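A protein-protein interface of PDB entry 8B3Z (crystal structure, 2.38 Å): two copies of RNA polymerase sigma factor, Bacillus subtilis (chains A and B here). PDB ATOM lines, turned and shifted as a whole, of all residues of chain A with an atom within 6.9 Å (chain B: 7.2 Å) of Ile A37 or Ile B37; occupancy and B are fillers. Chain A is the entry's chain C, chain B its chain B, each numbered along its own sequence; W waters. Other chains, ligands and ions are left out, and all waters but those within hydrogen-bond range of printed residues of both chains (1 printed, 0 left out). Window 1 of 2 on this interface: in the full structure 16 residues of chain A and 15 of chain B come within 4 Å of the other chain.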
ATOM      1  N   LEU A  16     -28.643   9.517  17.409  1.00  0.00           N
ATOM      2  CA  LEU A  16     -27.829  10.645  16.965  1.00  0.00           C
ATOM      3  C   LEU A  16     -26.601  10.165  16.206  1.00  0.00           C
ATOM      4  O   LEU A  16     -26.172  10.803  15.236  1.00  0.00           O
ATOM      5  CB  LEU A  16     -27.412  11.502  18.156  1.00  0.00           C
ATOM      6  CG  LEU A  16     -28.559  12.154  18.923  1.00  0.00           C
ATOM      7  CD1 LEU A  16     -28.014  13.181  19.907  1.00  0.00           C
ATOM      8  CD2 LEU A  16     -29.553  12.781  17.967  1.00  0.00           C
ATOM      9  N   VAL A  19     -26.779   9.797  12.457  1.00  0.00           N
ATOM     10  CA  VAL A  19     -26.567  10.990  11.639  1.00  0.00           C
ATOM     11  C   VAL A  19     -25.097  11.128  11.274  1.00  0.00           C
ATOM     12  O   VAL A  19     -24.752  11.435  10.128  1.00  0.00           O
ATOM     13  CB  VAL A  19     -27.071  12.250  12.364  1.00  0.00           C
ATOM     14  CG1 VAL A  19     -26.782  13.475  11.513  1.00  0.00           C
ATOM     15  CG2 VAL A  19     -28.565  12.143  12.681  1.00  0.00           C
ATOM     16  N   VAL A  20     -24.207  10.902  12.245  1.00  0.00           N
ATOM     17  CA  VAL A  20     -22.777  11.008  11.976  1.00  0.00           C
ATOM     18  C   VAL A  20     -22.349   9.961  10.958  1.00  0.00           C
ATOM     19  O   VAL A  20     -21.598  10.255  10.022  1.00  0.00           O
ATOM     20  CB  VAL A  20     -21.975  10.890  13.287  1.00  0.00           C
ATOM     21  CG1 VAL A  20     -20.502  10.831  12.984  1.00  0.00           C
ATOM     22  CG2 VAL A  20     -22.274  12.071  14.211  1.00  0.00           C
ATOM     23  N   ALA A  23     -23.583  11.042   7.545  1.00  0.00           N
ATOM     24  CA  ALA A  23     -22.965  12.279   7.076  1.00  0.00           C
ATOM     25  C   ALA A  23     -21.526  12.065   6.624  1.00  0.00           C
ATOM     26  O   ALA A  23     -21.078  12.712   5.671  1.00  0.00           O
ATOM     27  CB  ALA A  23     -23.025  13.347   8.165  1.00  0.00           C
ATOM     28  N   ARG A  24     -20.791  11.159   7.278  1.00  0.00           N
ATOM     29  CA  ARG A  24     -19.414  10.894   6.872  1.00  0.00           C
ATOM     30  C   ARG A  24     -19.319  10.264   5.489  1.00  0.00           C
ATOM     31  O   ARG A  24     -18.244  10.303   4.882  1.00  0.00           O
ATOM     32  CB  ARG A  24     -18.716  10.005   7.902  1.00  0.00           C
ATOM     33  CG  ARG A  24     -18.649  10.660   9.263  1.00  0.00           C
ATOM     34  CD  ARG A  24     -17.380  10.343  10.024  1.00  0.00           C
ATOM     35  NE  ARG A  24     -17.139  11.358  11.046  1.00  0.00           N
ATOM     36  CZ  ARG A  24     -16.551  12.526  10.815  1.00  0.00           C
ATOM     37  NH1 ARG A  24     -16.118  12.824   9.600  1.00  0.00           N
ATOM     38  NH2 ARG A  24     -16.382  13.394  11.804  1.00  0.00           N
ATOM     39  N   ASN A  32     -18.347  21.175   5.118  1.00  0.00           N
ATOM     40  CA  ASN A  32     -18.082  21.054   6.545  1.00  0.00           C
ATOM     41  C   ASN A  32     -18.977  19.994   7.178  1.00  0.00           C
ATOM     42  O   ASN A  32     -20.202  20.041   7.048  1.00  0.00           O
ATOM     43  CB  ASN A  32     -18.311  22.420   7.201  1.00  0.00           C
ATOM     44  CG  ASN A  32     -17.709  22.521   8.588  1.00  0.00           C
ATOM     45  OD1 ASN A  32     -17.025  21.608   9.059  1.00  0.00           O
ATOM     46  ND2 ASN A  32     -17.963  23.642   9.253  1.00  0.00           N
ATOM     47  N   ILE A  33     -18.354  19.029   7.861  1.00  0.00           N
ATOM     48  CA  ILE A  33     -19.102  17.941   8.492  1.00  0.00           C
ATOM     49  C   ILE A  33     -20.090  18.477   9.524  1.00  0.00           C
ATOM     50  O   ILE A  33     -21.174  17.908   9.706  1.00  0.00           O
ATOM     51  CB  ILE A  33     -18.132  16.918   9.121  1.00  0.00           C
ATOM     52  CG1 ILE A  33     -18.898  15.718   9.673  1.00  0.00           C
ATOM     53  CG2 ILE A  33     -17.324  17.557  10.250  1.00  0.00           C
ATOM     54  CD1 ILE A  33     -19.666  14.958   8.635  1.00  0.00           C
ATOM     55  N   GLU A  34     -19.742  19.571  10.209  1.00  0.00           N
ATOM     56  CA  GLU A  34     -20.654  20.173  11.179  1.00  0.00           C
ATOM     57  C   GLU A  34     -21.986  20.530  10.531  1.00  0.00           C
ATOM     58  O   GLU A  34     -23.055  20.262  11.090  1.00  0.00           O
ATOM     59  CB  GLU A  34     -20.014  21.415  11.802  1.00  0.00           C
ATOM     60  CG  GLU A  34     -18.662  21.181  12.471  1.00  0.00           C
ATOM     61  CD  GLU A  34     -18.002  22.474  12.943  1.00  0.00           C
ATOM     62  OE1 GLU A  34     -18.002  23.471  12.190  1.00  0.00           O
ATOM     63  OE2 GLU A  34     -17.487  22.498  14.080  1.00  0.00           O
ATOM     64  N   ASP A  35     -21.945  21.130   9.339  1.00  0.00           N
ATOM     65  CA  ASP A  35     -23.189  21.516   8.682  1.00  0.00           C
ATOM     66  C   ASP A  35     -23.979  20.294   8.229  1.00  0.00           C
ATOM     67  O   ASP A  35     -25.212  20.266   8.346  1.00  0.00           O
ATOM     68  CB  ASP A  35     -22.894  22.446   7.509  1.00  0.00           C
ATOM     69  CG  ASP A  35     -22.287  23.768   7.957  1.00  0.00           C
ATOM     70  OD1 ASP A  35     -22.290  24.035   9.179  1.00  0.00           O
ATOM     71  OD2 ASP A  35     -21.797  24.533   7.096  1.00  0.00           O
ATOM     72  N   LEU A  36     -23.286  19.267   7.734  1.00  0.00           N
ATOM     73  CA  LEU A  36     -23.976  18.048   7.328  1.00  0.00           C
ATOM     74  C   LEU A  36     -24.689  17.403   8.509  1.00  0.00           C
ATOM     75  O   LEU A  36     -25.842  16.966   8.388  1.00  0.00           O
ATOM     76  CB  LEU A  36     -22.985  17.076   6.692  1.00  0.00           C
ATOM     77  CG  LEU A  36     -22.382  17.559   5.373  1.00  0.00           C
ATOM     78  CD1 LEU A  36     -21.419  16.530   4.807  1.00  0.00           C
ATOM     79  CD2 LEU A  36     -23.489  17.852   4.381  1.00  0.00           C
ATOM     80  N   ILE A  37     -24.024  17.342   9.664  1.00  0.00           N
ATOM     81  CA  ILE A  37     -24.629  16.738  10.847  1.00  0.00           C
ATOM     82  C   ILE A  37     -25.905  17.476  11.221  1.00  0.00           C
ATOM     83  O   ILE A  37     -26.944  16.864  11.491  1.00  0.00           O
ATOM     84  CB  ILE A  37     -23.623  16.714  12.011  1.00  0.00           C
ATOM     85  CG1 ILE A  37     -22.566  15.629  11.754  1.00  0.00           C
ATOM     86  CG2 ILE A  37     -24.351  16.525  13.344  1.00  0.00           C
ATOM     87  CD1 ILE A  37     -21.372  15.714  12.666  1.00  0.00           C
ATOM     88  N   SER A  38     -25.849  18.805  11.212  1.00  0.00           N
ATOM     89  CA  SER A  38     -27.043  19.593  11.504  1.00  0.00           C
ATOM     90  C   SER A  38     -28.149  19.300  10.500  1.00  0.00           C
ATOM     91  O   SER A  38     -29.302  19.057  10.884  1.00  0.00           O
ATOM     92  CB  SER A  38     -26.690  21.078  11.509  1.00  0.00           C
ATOM     93  OG  SER A  38     -27.666  21.811  12.217  1.00  0.00           O
ATOM     94  N   ILE A  39     -27.814  19.297   9.204  1.00  0.00           N
ATOM     95  CA  ILE A  39     -28.804  19.017   8.164  1.00  0.00           C
ATOM     96  C   ILE A  39     -29.365  17.612   8.331  1.00  0.00           C
ATOM     97  O   ILE A  39     -30.581  17.392   8.273  1.00  0.00           O
ATOM     98  CB  ILE A  39     -28.185  19.208   6.769  1.00  0.00           C
ATOM     99  CG1 ILE A  39     -27.951  20.695   6.496  1.00  0.00           C
ATOM    100  CG2 ILE A  39     -29.079  18.597   5.696  1.00  0.00           C
ATOM    101  CD1 ILE A  39     -29.253  21.484   6.400  1.00  0.00           C
ATOM    102  N   GLY A  40     -28.480  16.640   8.549  1.00  0.00           N
ATOM    103  CA  GLY A  40     -28.933  15.275   8.742  1.00  0.00           C
ATOM    104  C   GLY A  40     -29.812  15.110   9.961  1.00  0.00           C
ATOM    105  O   GLY A  40     -30.714  14.266   9.970  1.00  0.00           O
ATOM    106  N   THR A  41     -29.564  15.898  11.013  1.00  0.00           N
ATOM    107  CA  THR A  41     -30.418  15.820  12.190  1.00  0.00           C
ATOM    108  C   THR A  41     -31.851  16.191  11.836  1.00  0.00           C
ATOM    109  O   THR A  41     -32.800  15.555  12.311  1.00  0.00           O
ATOM    110  CB  THR A  41     -29.886  16.725  13.304  1.00  0.00           C
ATOM    111  OG1 THR A  41     -28.531  16.371  13.610  1.00  0.00           O
ATOM    112  CG2 THR A  41     -30.733  16.568  14.564  1.00  0.00           C
ATOM    113  N   ILE A  42     -32.022  17.218  10.993  1.00  0.00           N
ATOM    114  CA  ILE A  42     -33.348  17.561  10.474  1.00  0.00           C
ATOM    115  C   ILE A  42     -33.992  16.339   9.833  1.00  0.00           C
ATOM    116  O   ILE A  42     -35.165  16.024  10.081  1.00  0.00           O
ATOM    117  CB  ILE A  42     -33.239  18.728   9.476  1.00  0.00           C
ATOM    118  CG1 ILE A  42     -32.735  19.989  10.180  1.00  0.00           C
ATOM    119  CG2 ILE A  42     -34.570  18.970   8.765  1.00  0.00           C
ATOM    120  CD1 ILE A  42     -32.367  21.094   9.213  1.00  0.00           C
ATOM    121  N   GLY A  43     -33.227  15.620   9.012  1.00  0.00           N
ATOM    122  CA  GLY A  43     -33.745  14.394   8.430  1.00  0.00           C
ATOM    123  C   GLY A  43     -34.167  13.375   9.474  1.00  0.00           C
ATOM    124  O   GLY A  43     -35.201  12.719   9.328  1.00  0.00           O
ATOM    125  N   ILE A  67     -32.307  10.749   6.435  1.00  0.00           N
ATOM    126  CA  ILE A  67     -31.081  11.488   6.733  1.00  0.00           C
ATOM    127  C   ILE A  67     -30.255  11.687   5.470  1.00  0.00           C
ATOM    128  O   ILE A  67     -29.794  12.797   5.174  1.00  0.00           O
ATOM    129  CB  ILE A  67     -30.274  10.757   7.818  1.00  0.00           C
ATOM    130  CG1 ILE A  67     -31.016  10.787   9.153  1.00  0.00           C
ATOM    131  CG2 ILE A  67     -28.897  11.370   7.953  1.00  0.00           C
ATOM    132  CD1 ILE A  67     -30.519   9.745  10.121  1.00  0.00           C
ATOM    133  N   ILE A  71     -29.601  15.369   3.366  1.00  0.00           N
ATOM    134  CA  ILE A  71     -28.272  15.849   3.010  1.00  0.00           C
ATOM    135  C   ILE A  71     -28.149  16.004   1.501  1.00  0.00           C
ATOM    136  O   ILE A  71     -27.604  16.999   1.008  1.00  0.00           O
ATOM    137  CB  ILE A  71     -27.201  14.899   3.577  1.00  0.00           C
ATOM    138  CG1 ILE A  71     -27.237  14.931   5.114  1.00  0.00           C
ATOM    139  CG2 ILE A  71     -25.824  15.260   3.033  1.00  0.00           C
ATOM    140  CD1 ILE A  71     -26.221  14.037   5.787  1.00  0.00           C
ATOM    141  N   LEU B  16     -27.982  27.692  10.768  1.00  0.00           N
ATOM    142  CA  LEU B  16     -27.225  26.499  11.138  1.00  0.00           C
ATOM    143  C   LEU B  16     -25.913  26.856  11.820  1.00  0.00           C
ATOM    144  O   LEU B  16     -25.530  26.221  12.813  1.00  0.00           O
ATOM    145  CB  LEU B  16     -26.965  25.631   9.911  1.00  0.00           C
ATOM    146  CG  LEU B  16     -28.209  25.026   9.266  1.00  0.00           C
ATOM    147  CD1 LEU B  16     -27.768  24.108   8.158  1.00  0.00           C
ATOM    148  CD2 LEU B  16     -29.020  24.280  10.308  1.00  0.00           C
ATOM    149  N   VAL B  19     -26.164  27.221  15.466  1.00  0.00           N
ATOM    150  CA  VAL B  19     -26.144  25.961  16.207  1.00  0.00           C
ATOM    151  C   VAL B  19     -24.711  25.556  16.526  1.00  0.00           C
ATOM    152  O   VAL B  19     -24.384  25.196  17.663  1.00  0.00           O
ATOM    153  CB  VAL B  19     -26.858  24.852  15.413  1.00  0.00           C
ATOM    154  CG1 VAL B  19     -26.656  23.487  16.093  1.00  0.00           C
ATOM    155  CG2 VAL B  19     -28.326  25.166  15.250  1.00  0.00           C
ATOM    156  N   VAL B  20     -23.844  25.590  15.516  1.00  0.00           N
ATOM    157  CA  VAL B  20     -22.458  25.178  15.712  1.00  0.00           C
ATOM    158  C   VAL B  20     -21.773  26.097  16.711  1.00  0.00           C
ATOM    159  O   VAL B  20     -21.141  25.638  17.671  1.00  0.00           O
ATOM    160  CB  VAL B  20     -21.711  25.152  14.365  1.00  0.00           C
ATOM    161  CG1 VAL B  20     -20.262  24.772  14.579  1.00  0.00           C
ATOM    162  CG2 VAL B  20     -22.383  24.181  13.397  1.00  0.00           C
ATOM    163  N   TYR B  21     -21.909  27.412  16.512  1.00  0.00           N
ATOM    164  CA  TYR B  21     -21.238  28.380  17.375  1.00  0.00           C
ATOM    165  C   TYR B  21     -21.567  28.131  18.844  1.00  0.00           C
ATOM    166  O   TYR B  21     -20.674  28.115  19.700  1.00  0.00           O
ATOM    167  CB  TYR B  21     -21.635  29.797  16.966  1.00  0.00           C
ATOM    168  CG  TYR B  21     -20.916  30.878  17.734  1.00  0.00           C
ATOM    169  CD1 TYR B  21     -19.557  31.103  17.548  1.00  0.00           C
ATOM    170  CD2 TYR B  21     -21.593  31.677  18.646  1.00  0.00           C
ATOM    171  CE1 TYR B  21     -18.895  32.093  18.245  1.00  0.00           C
ATOM    172  CE2 TYR B  21     -20.941  32.672  19.351  1.00  0.00           C
ATOM    173  CZ  TYR B  21     -19.592  32.875  19.145  1.00  0.00           C
ATOM    174  OH  TYR B  21     -18.934  33.861  19.845  1.00  0.00           O
ATOM    175  N   ALA B  23     -22.797  25.302  20.078  1.00  0.00           N
ATOM    176  CA  ALA B  23     -22.379  23.959  20.463  1.00  0.00           C
ATOM    177  C   ALA B  23     -20.914  23.936  20.879  1.00  0.00           C
ATOM    178  O   ALA B  23     -20.540  23.225  21.818  1.00  0.00           O
ATOM    179  CB  ALA B  23     -22.626  22.982  19.318  1.00  0.00           C
ATOM    180  N   ARG B  24     -20.070  24.716  20.197  1.00  0.00           N
ATOM    181  CA  ARG B  24     -18.650  24.712  20.527  1.00  0.00           C
ATOM    182  C   ARG B  24     -18.392  25.275  21.918  1.00  0.00           C
ATOM    183  O   ARG B  24     -17.426  24.873  22.575  1.00  0.00           O
ATOM    184  CB  ARG B  24     -17.859  25.484  19.473  1.00  0.00           C
ATOM    185  CG  ARG B  24     -18.205  25.090  18.046  1.00  0.00           C
ATOM    186  CD  ARG B  24     -17.033  24.476  17.301  1.00  0.00           C
ATOM    187  NE  ARG B  24     -16.702  23.140  17.784  1.00  0.00           N
ATOM    188  CZ  ARG B  24     -15.910  22.289  17.138  1.00  0.00           C
ATOM    189  NH1 ARG B  24     -15.378  22.633  15.975  1.00  0.00           N
ATOM    190  NH2 ARG B  24     -15.655  21.092  17.649  1.00  0.00           N
ATOM    191  N   ASN B  32     -19.335  15.307  23.444  1.00  0.00           N
ATOM    192  CA  ASN B  32     -18.891  15.305  22.057  1.00  0.00           C
ATOM    193  C   ASN B  32     -19.636  16.342  21.225  1.00  0.00           C
ATOM    194  O   ASN B  32     -20.866  16.448  21.279  1.00  0.00           O
ATOM    195  CB  ASN B  32     -19.066  13.933  21.424  1.00  0.00           C
ATOM    196  CG  ASN B  32     -18.849  13.972  19.926  1.00  0.00           C
ATOM    197  OD1 ASN B  32     -19.707  13.543  19.157  1.00  0.00           O
ATOM    198  ND2 ASN B  32     -17.705  14.497  19.500  1.00  0.00           N
ATOM    199  N   ILE B  33     -18.870  17.089  20.426  1.00  0.00           N
ATOM    200  CA  ILE B  33     -19.421  18.195  19.652  1.00  0.00           C
ATOM    201  C   ILE B  33     -20.522  17.724  18.710  1.00  0.00           C
ATOM    202  O   ILE B  33     -21.479  18.463  18.447  1.00  0.00           O
ATOM    203  CB  ILE B  33     -18.287  18.908  18.890  1.00  0.00           C
ATOM    204  CG1 ILE B  33     -18.833  20.134  18.153  1.00  0.00           C
ATOM    205  CG2 ILE B  33     -17.581  17.938  17.945  1.00  0.00           C
ATOM    206  CD1 ILE B  33     -19.500  21.133  19.073  1.00  0.00           C
ATOM    207  N   GLU B  34     -20.421  16.495  18.200  1.00  0.00           N
ATOM    208  CA  GLU B  34     -21.402  16.017  17.229  1.00  0.00           C
ATOM    209  C   GLU B  34     -22.760  15.798  17.879  1.00  0.00           C
ATOM    210  O   GLU B  34     -23.800  16.050  17.256  1.00  0.00           O
ATOM    211  CB  GLU B  34     -20.907  14.732  16.566  1.00  0.00           C
ATOM    212  CG  GLU B  34     -19.535  14.861  15.936  1.00  0.00           C
ATOM    213  CD  GLU B  34     -18.864  13.520  15.733  1.00  0.00           C
ATOM    214  OE1 GLU B  34     -19.080  12.608  16.559  1.00  0.00           O
ATOM    215  OE2 GLU B  34     -18.121  13.377  14.741  1.00  0.00           O
ATOM    216  N   ASP B  35     -22.772  15.312  19.123  1.00  0.00           N
ATOM    217  CA  ASP B  35     -24.016  15.254  19.881  1.00  0.00           C
ATOM    218  C   ASP B  35     -24.589  16.648  20.099  1.00  0.00           C
ATOM    219  O   ASP B  35     -25.799  16.861  19.960  1.00  0.00           O
ATOM    220  CB  ASP B  35     -23.778  14.571  21.226  1.00  0.00           C
ATOM    221  CG  ASP B  35     -23.441  13.109  21.085  1.00  0.00           C
ATOM    222  OD1 ASP B  35     -23.844  12.506  20.072  1.00  0.00           O
ATOM    223  OD2 ASP B  35     -22.786  12.560  21.996  1.00  0.00           O
ATOM    224  N   LEU B  36     -23.728  17.613  20.435  1.00  0.00           N
ATOM    225  CA  LEU B  36     -24.203  18.954  20.759  1.00  0.00           C
ATOM    226  C   LEU B  36     -24.760  19.659  19.531  1.00  0.00           C
ATOM    227  O   LEU B  36     -25.717  20.431  19.645  1.00  0.00           O
ATOM    228  CB  LEU B  36     -23.072  19.776  21.380  1.00  0.00           C
ATOM    229  CG  LEU B  36     -22.530  19.244  22.710  1.00  0.00           C
ATOM    230  CD1 LEU B  36     -21.263  19.985  23.130  1.00  0.00           C
ATOM    231  CD2 LEU B  36     -23.595  19.360  23.785  1.00  0.00           C
ATOM    232  N   ILE B  37     -24.178  19.414  18.356  1.00  0.00           N
ATOM    233  CA  ILE B  37     -24.735  19.987  17.137  1.00  0.00           C
ATOM    234  C   ILE B  37     -26.131  19.431  16.888  1.00  0.00           C
ATOM    235  O   ILE B  37     -27.080  20.176  16.621  1.00  0.00           O
ATOM    236  CB  ILE B  37     -23.796  19.728  15.951  1.00  0.00           C
ATOM    237  CG1 ILE B  37     -22.502  20.528  16.134  1.00  0.00           C
ATOM    238  CG2 ILE B  37     -24.486  20.079  14.642  1.00  0.00           C
ATOM    239  CD1 ILE B  37     -21.423  20.155  15.146  1.00  0.00           C
ATOM    240  N   SER B  38     -26.286  18.114  17.015  1.00  0.00           N
ATOM    241  CA  SER B  38     -27.599  17.511  16.830  1.00  0.00           C
ATOM    242  C   SER B  38     -28.607  18.088  17.814  1.00  0.00           C
ATOM    243  O   SER B  38     -29.661  18.595  17.413  1.00  0.00           O
ATOM    244  CB  SER B  38     -27.499  16.001  16.992  1.00  0.00           C
ATOM    245  OG  SER B  38     -27.181  15.397  15.756  1.00  0.00           O
ATOM    246  N   ILE B  39     -28.288  18.014  19.113  1.00  0.00           N
ATOM    247  CA  ILE B  39     -29.179  18.521  20.155  1.00  0.00           C
ATOM    248  C   ILE B  39     -29.496  19.990  19.914  1.00  0.00           C
ATOM    249  O   ILE B  39     -30.656  20.417  19.989  1.00  0.00           O
ATOM    250  CB  ILE B  39     -28.546  18.315  21.544  1.00  0.00           C
ATOM    251  CG1 ILE B  39     -28.425  16.823  21.889  1.00  0.00           C
ATOM    252  CG2 ILE B  39     -29.327  19.094  22.605  1.00  0.00           C
ATOM    253  CD1 ILE B  39     -29.743  16.066  21.922  1.00  0.00           C
ATOM    254  N   GLY B  40     -28.465  20.786  19.623  1.00  0.00           N
ATOM    255  CA  GLY B  40     -28.680  22.201  19.381  1.00  0.00           C
ATOM    256  C   GLY B  40     -29.575  22.447  18.185  1.00  0.00           C
ATOM    257  O   GLY B  40     -30.427  23.339  18.212  1.00  0.00           O
ATOM    258  N   THR B  41     -29.399  21.651  17.123  1.00  0.00           N
ATOM    259  CA  THR B  41     -30.275  21.750  15.958  1.00  0.00           C
ATOM    260  C   THR B  41     -31.728  21.519  16.347  1.00  0.00           C
ATOM    261  O   THR B  41     -32.639  22.158  15.804  1.00  0.00           O
ATOM    262  CB  THR B  41     -29.850  20.740  14.893  1.00  0.00           C
ATOM    263  OG1 THR B  41     -28.524  21.046  14.450  1.00  0.00           O
ATOM    264  CG2 THR B  41     -30.804  20.771  13.700  1.00  0.00           C
ATOM    265  N   ILE B  42     -31.966  20.616  17.292  1.00  0.00           N
ATOM    266  CA  ILE B  42     -33.329  20.405  17.767  1.00  0.00           C
ATOM    267  C   ILE B  42     -33.881  21.689  18.374  1.00  0.00           C
ATOM    268  O   ILE B  42     -35.051  22.038  18.166  1.00  0.00           O
ATOM    269  CB  ILE B  42     -33.360  19.227  18.756  1.00  0.00           C
ATOM    270  CG1 ILE B  42     -32.989  17.938  18.018  1.00  0.00           C
ATOM    271  CG2 ILE B  42     -34.711  19.136  19.467  1.00  0.00           C
ATOM    272  CD1 ILE B  42     -32.831  16.746  18.930  1.00  0.00           C
ATOM    273  N   GLY B  43     -33.048  22.421  19.120  1.00  0.00           N
ATOM    274  CA  GLY B  43     -33.504  23.680  19.691  1.00  0.00           C
ATOM    275  C   GLY B  43     -33.810  24.716  18.624  1.00  0.00           C
ATOM    276  O   GLY B  43     -34.755  25.498  18.754  1.00  0.00           O
ATOM    277  N   ILE B  67     -31.587  27.153  21.535  1.00  0.00           N
ATOM    278  CA  ILE B  67     -30.478  26.236  21.299  1.00  0.00           C
ATOM    279  C   ILE B  67     -29.735  25.959  22.600  1.00  0.00           C
ATOM    280  O   ILE B  67     -29.491  24.798  22.962  1.00  0.00           O
ATOM    281  CB  ILE B  67     -29.539  26.811  20.225  1.00  0.00           C
ATOM    282  CG1 ILE B  67     -30.261  26.901  18.877  1.00  0.00           C
ATOM    283  CG2 ILE B  67     -28.274  25.975  20.102  1.00  0.00           C
ATOM    284  CD1 ILE B  67     -29.643  27.888  17.945  1.00  0.00           C
ATOM    285  N   ILE B  71     -29.565  22.316  24.803  1.00  0.00           N
ATOM    286  CA  ILE B  71     -28.293  21.711  25.181  1.00  0.00           C
ATOM    287  C   ILE B  71     -28.196  21.558  26.695  1.00  0.00           C
ATOM    288  O   ILE B  71     -27.792  20.500  27.198  1.00  0.00           O
ATOM    289  CB  ILE B  71     -27.126  22.538  24.610  1.00  0.00           C
ATOM    290  CG1 ILE B  71     -26.983  22.270  23.103  1.00  0.00           C
ATOM    291  CG2 ILE B  71     -25.833  22.225  25.372  1.00  0.00           C
ATOM    292  CD1 ILE B  71     -25.995  23.174  22.380  1.00  0.00           C
HETATM  293  O   HOH W   1     -25.002  13.519  15.990  1.00  0.00           O
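NH1 of Arg B24 lies within salt-bridge range of OE2 of Glu A34.
OE2 of Glu B34 is in salt-bridge range of NH2 of Arg A24.
The side-chain hydroxyl (OG) of Ser B38 is in hydrogen-bond range of the side-chain hydroxyl (OG1) of Thr A41 (2.7 Å).
OG1 of Thr B41 lies within hydrogen-bond range of OG of Ser A38, 2.5 Å away.
The side-chain amide oxygen of Asn B32 lies close to the side-chain carboxylate of Glu B34.
The backbone carbonyl oxygen (O) of Ile B37 sits at hydrogen-bond distance from the side-chain hydroxyl (OG1) of Thr B41 (2.7 Å).
The side-chain amide nitrogen (ND2) of Asn A32 sits at hydrogen-bond distance from the side-chain carboxylate (OE1) of Glu A34.
OG1 of Thr A41 sits at hydrogen-bond distance from O of Ile A37 (2.7 Å).
Among the printed residues, merely in contact across the chains: Leu A16 with Ser B38 (3.9 Å), Leu A16 with Ile B39 (3.9 Å), Val A20 with Glu B34 (3.8 Å), Glu A34 with Val B20 (3.5 Å), Glu A34 with Ile B37 (3.8 Å), Ile A37 with Glu B34 (3.8 Å), Ile A37 with Ile B37 (3.8 Å), Ile A37 with Ser B38 (3.9 Å), Ser A38 with Leu B16 (3.4 Å), Ser A38 with Ile B37 (3.9 Å) and Ile A39 with Leu B16 (3.5 Å).
Ile A37 touches just these residues of chain B: Glu B34 (3.8 Å), Ile B37 (3.8 Å) and Ser B38 (3.9 Å).
Ile B37 touches just these residues of chain A: Glu A34 (3.8 Å), Ile A37 (3.8 Å) and Ser A38 (3.9 Å).
Of the printed residues of chain B, Ser A38 touches Leu B16, Ile B37 and Thr B41.
Of the printed residues of chain A, Ile B39 touches Leu A16 (3.9 Å).
Of the printed residues of chain A, Arg B24 touches Glu A34 (2.8 Å).
Printed residues of chain A within 4 Å of Leu B16: Ser A38 (3.4 Å) and Ile A39 (3.5 Å).
Of the printed residues of chain B, Arg A24 touches Glu B34 (3.4 Å).
Ile B42 touches none of the printed residues of chain A.
Val A19 touches none of the printed residues of chain B.
The nearest residue of chain B that does not touch Ile A37 is Thr B41 (5.4 Å).
Hydrophobic or aromatic side chains of chain B within 4 Å of the printed part of chain A: Leu B16, Val B20, Ile B37 and Ile B39.
Printed residues of chain A that touch a printed residue of chain B: Leu A16, Val A20, Arg A24, Glu A34, Ile A37, Ser A38, Ile A39 and Thr A41.
Hydrophobic or aromatic side chains of chain A that line the printed part of chain B: Leu A16, Val A20, Ile A37 and Ile A39.
Among the printed residues, 15 pairs touch across the chains.
Among the printed residues, Asp or Glu carboxylates within 4 Å of a Lys or Arg side-chain nitrogen of the other chain: Arg A24 with Glu B34 (3.4 Å) and Glu A34 with Arg B24 (2.8 Å).
Leu A16 touches Ser B38, and with the chains exchanged Ser A38 touches Leu B16.
Leu A16 touches Ile B39, and with the chains exchanged Ile A39 touches Leu B16.
Val A20 touches Glu B34, and with the chains exchanged Glu A34 touches Val B20.
Ser A38 touches Thr B41, and with the chains exchanged Thr A41 touches Ser B38.
Positions printed for both chains: 16, 19, 20, 23, 24, 32, 33, 34, 35, 36, 37, 38, 39, 40, 41, 42, 43, 67 and 71.
Water W1 lies within hydrogen-bond range of the side-chain hydroxyl (OG) of Ser B38 (2.9 Å), the backbone carbonyl oxygen (O) of Leu A16 (3.1 Å) and the backbone carbonyl oxygen (O) of Glu B34 (3.1 Å).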
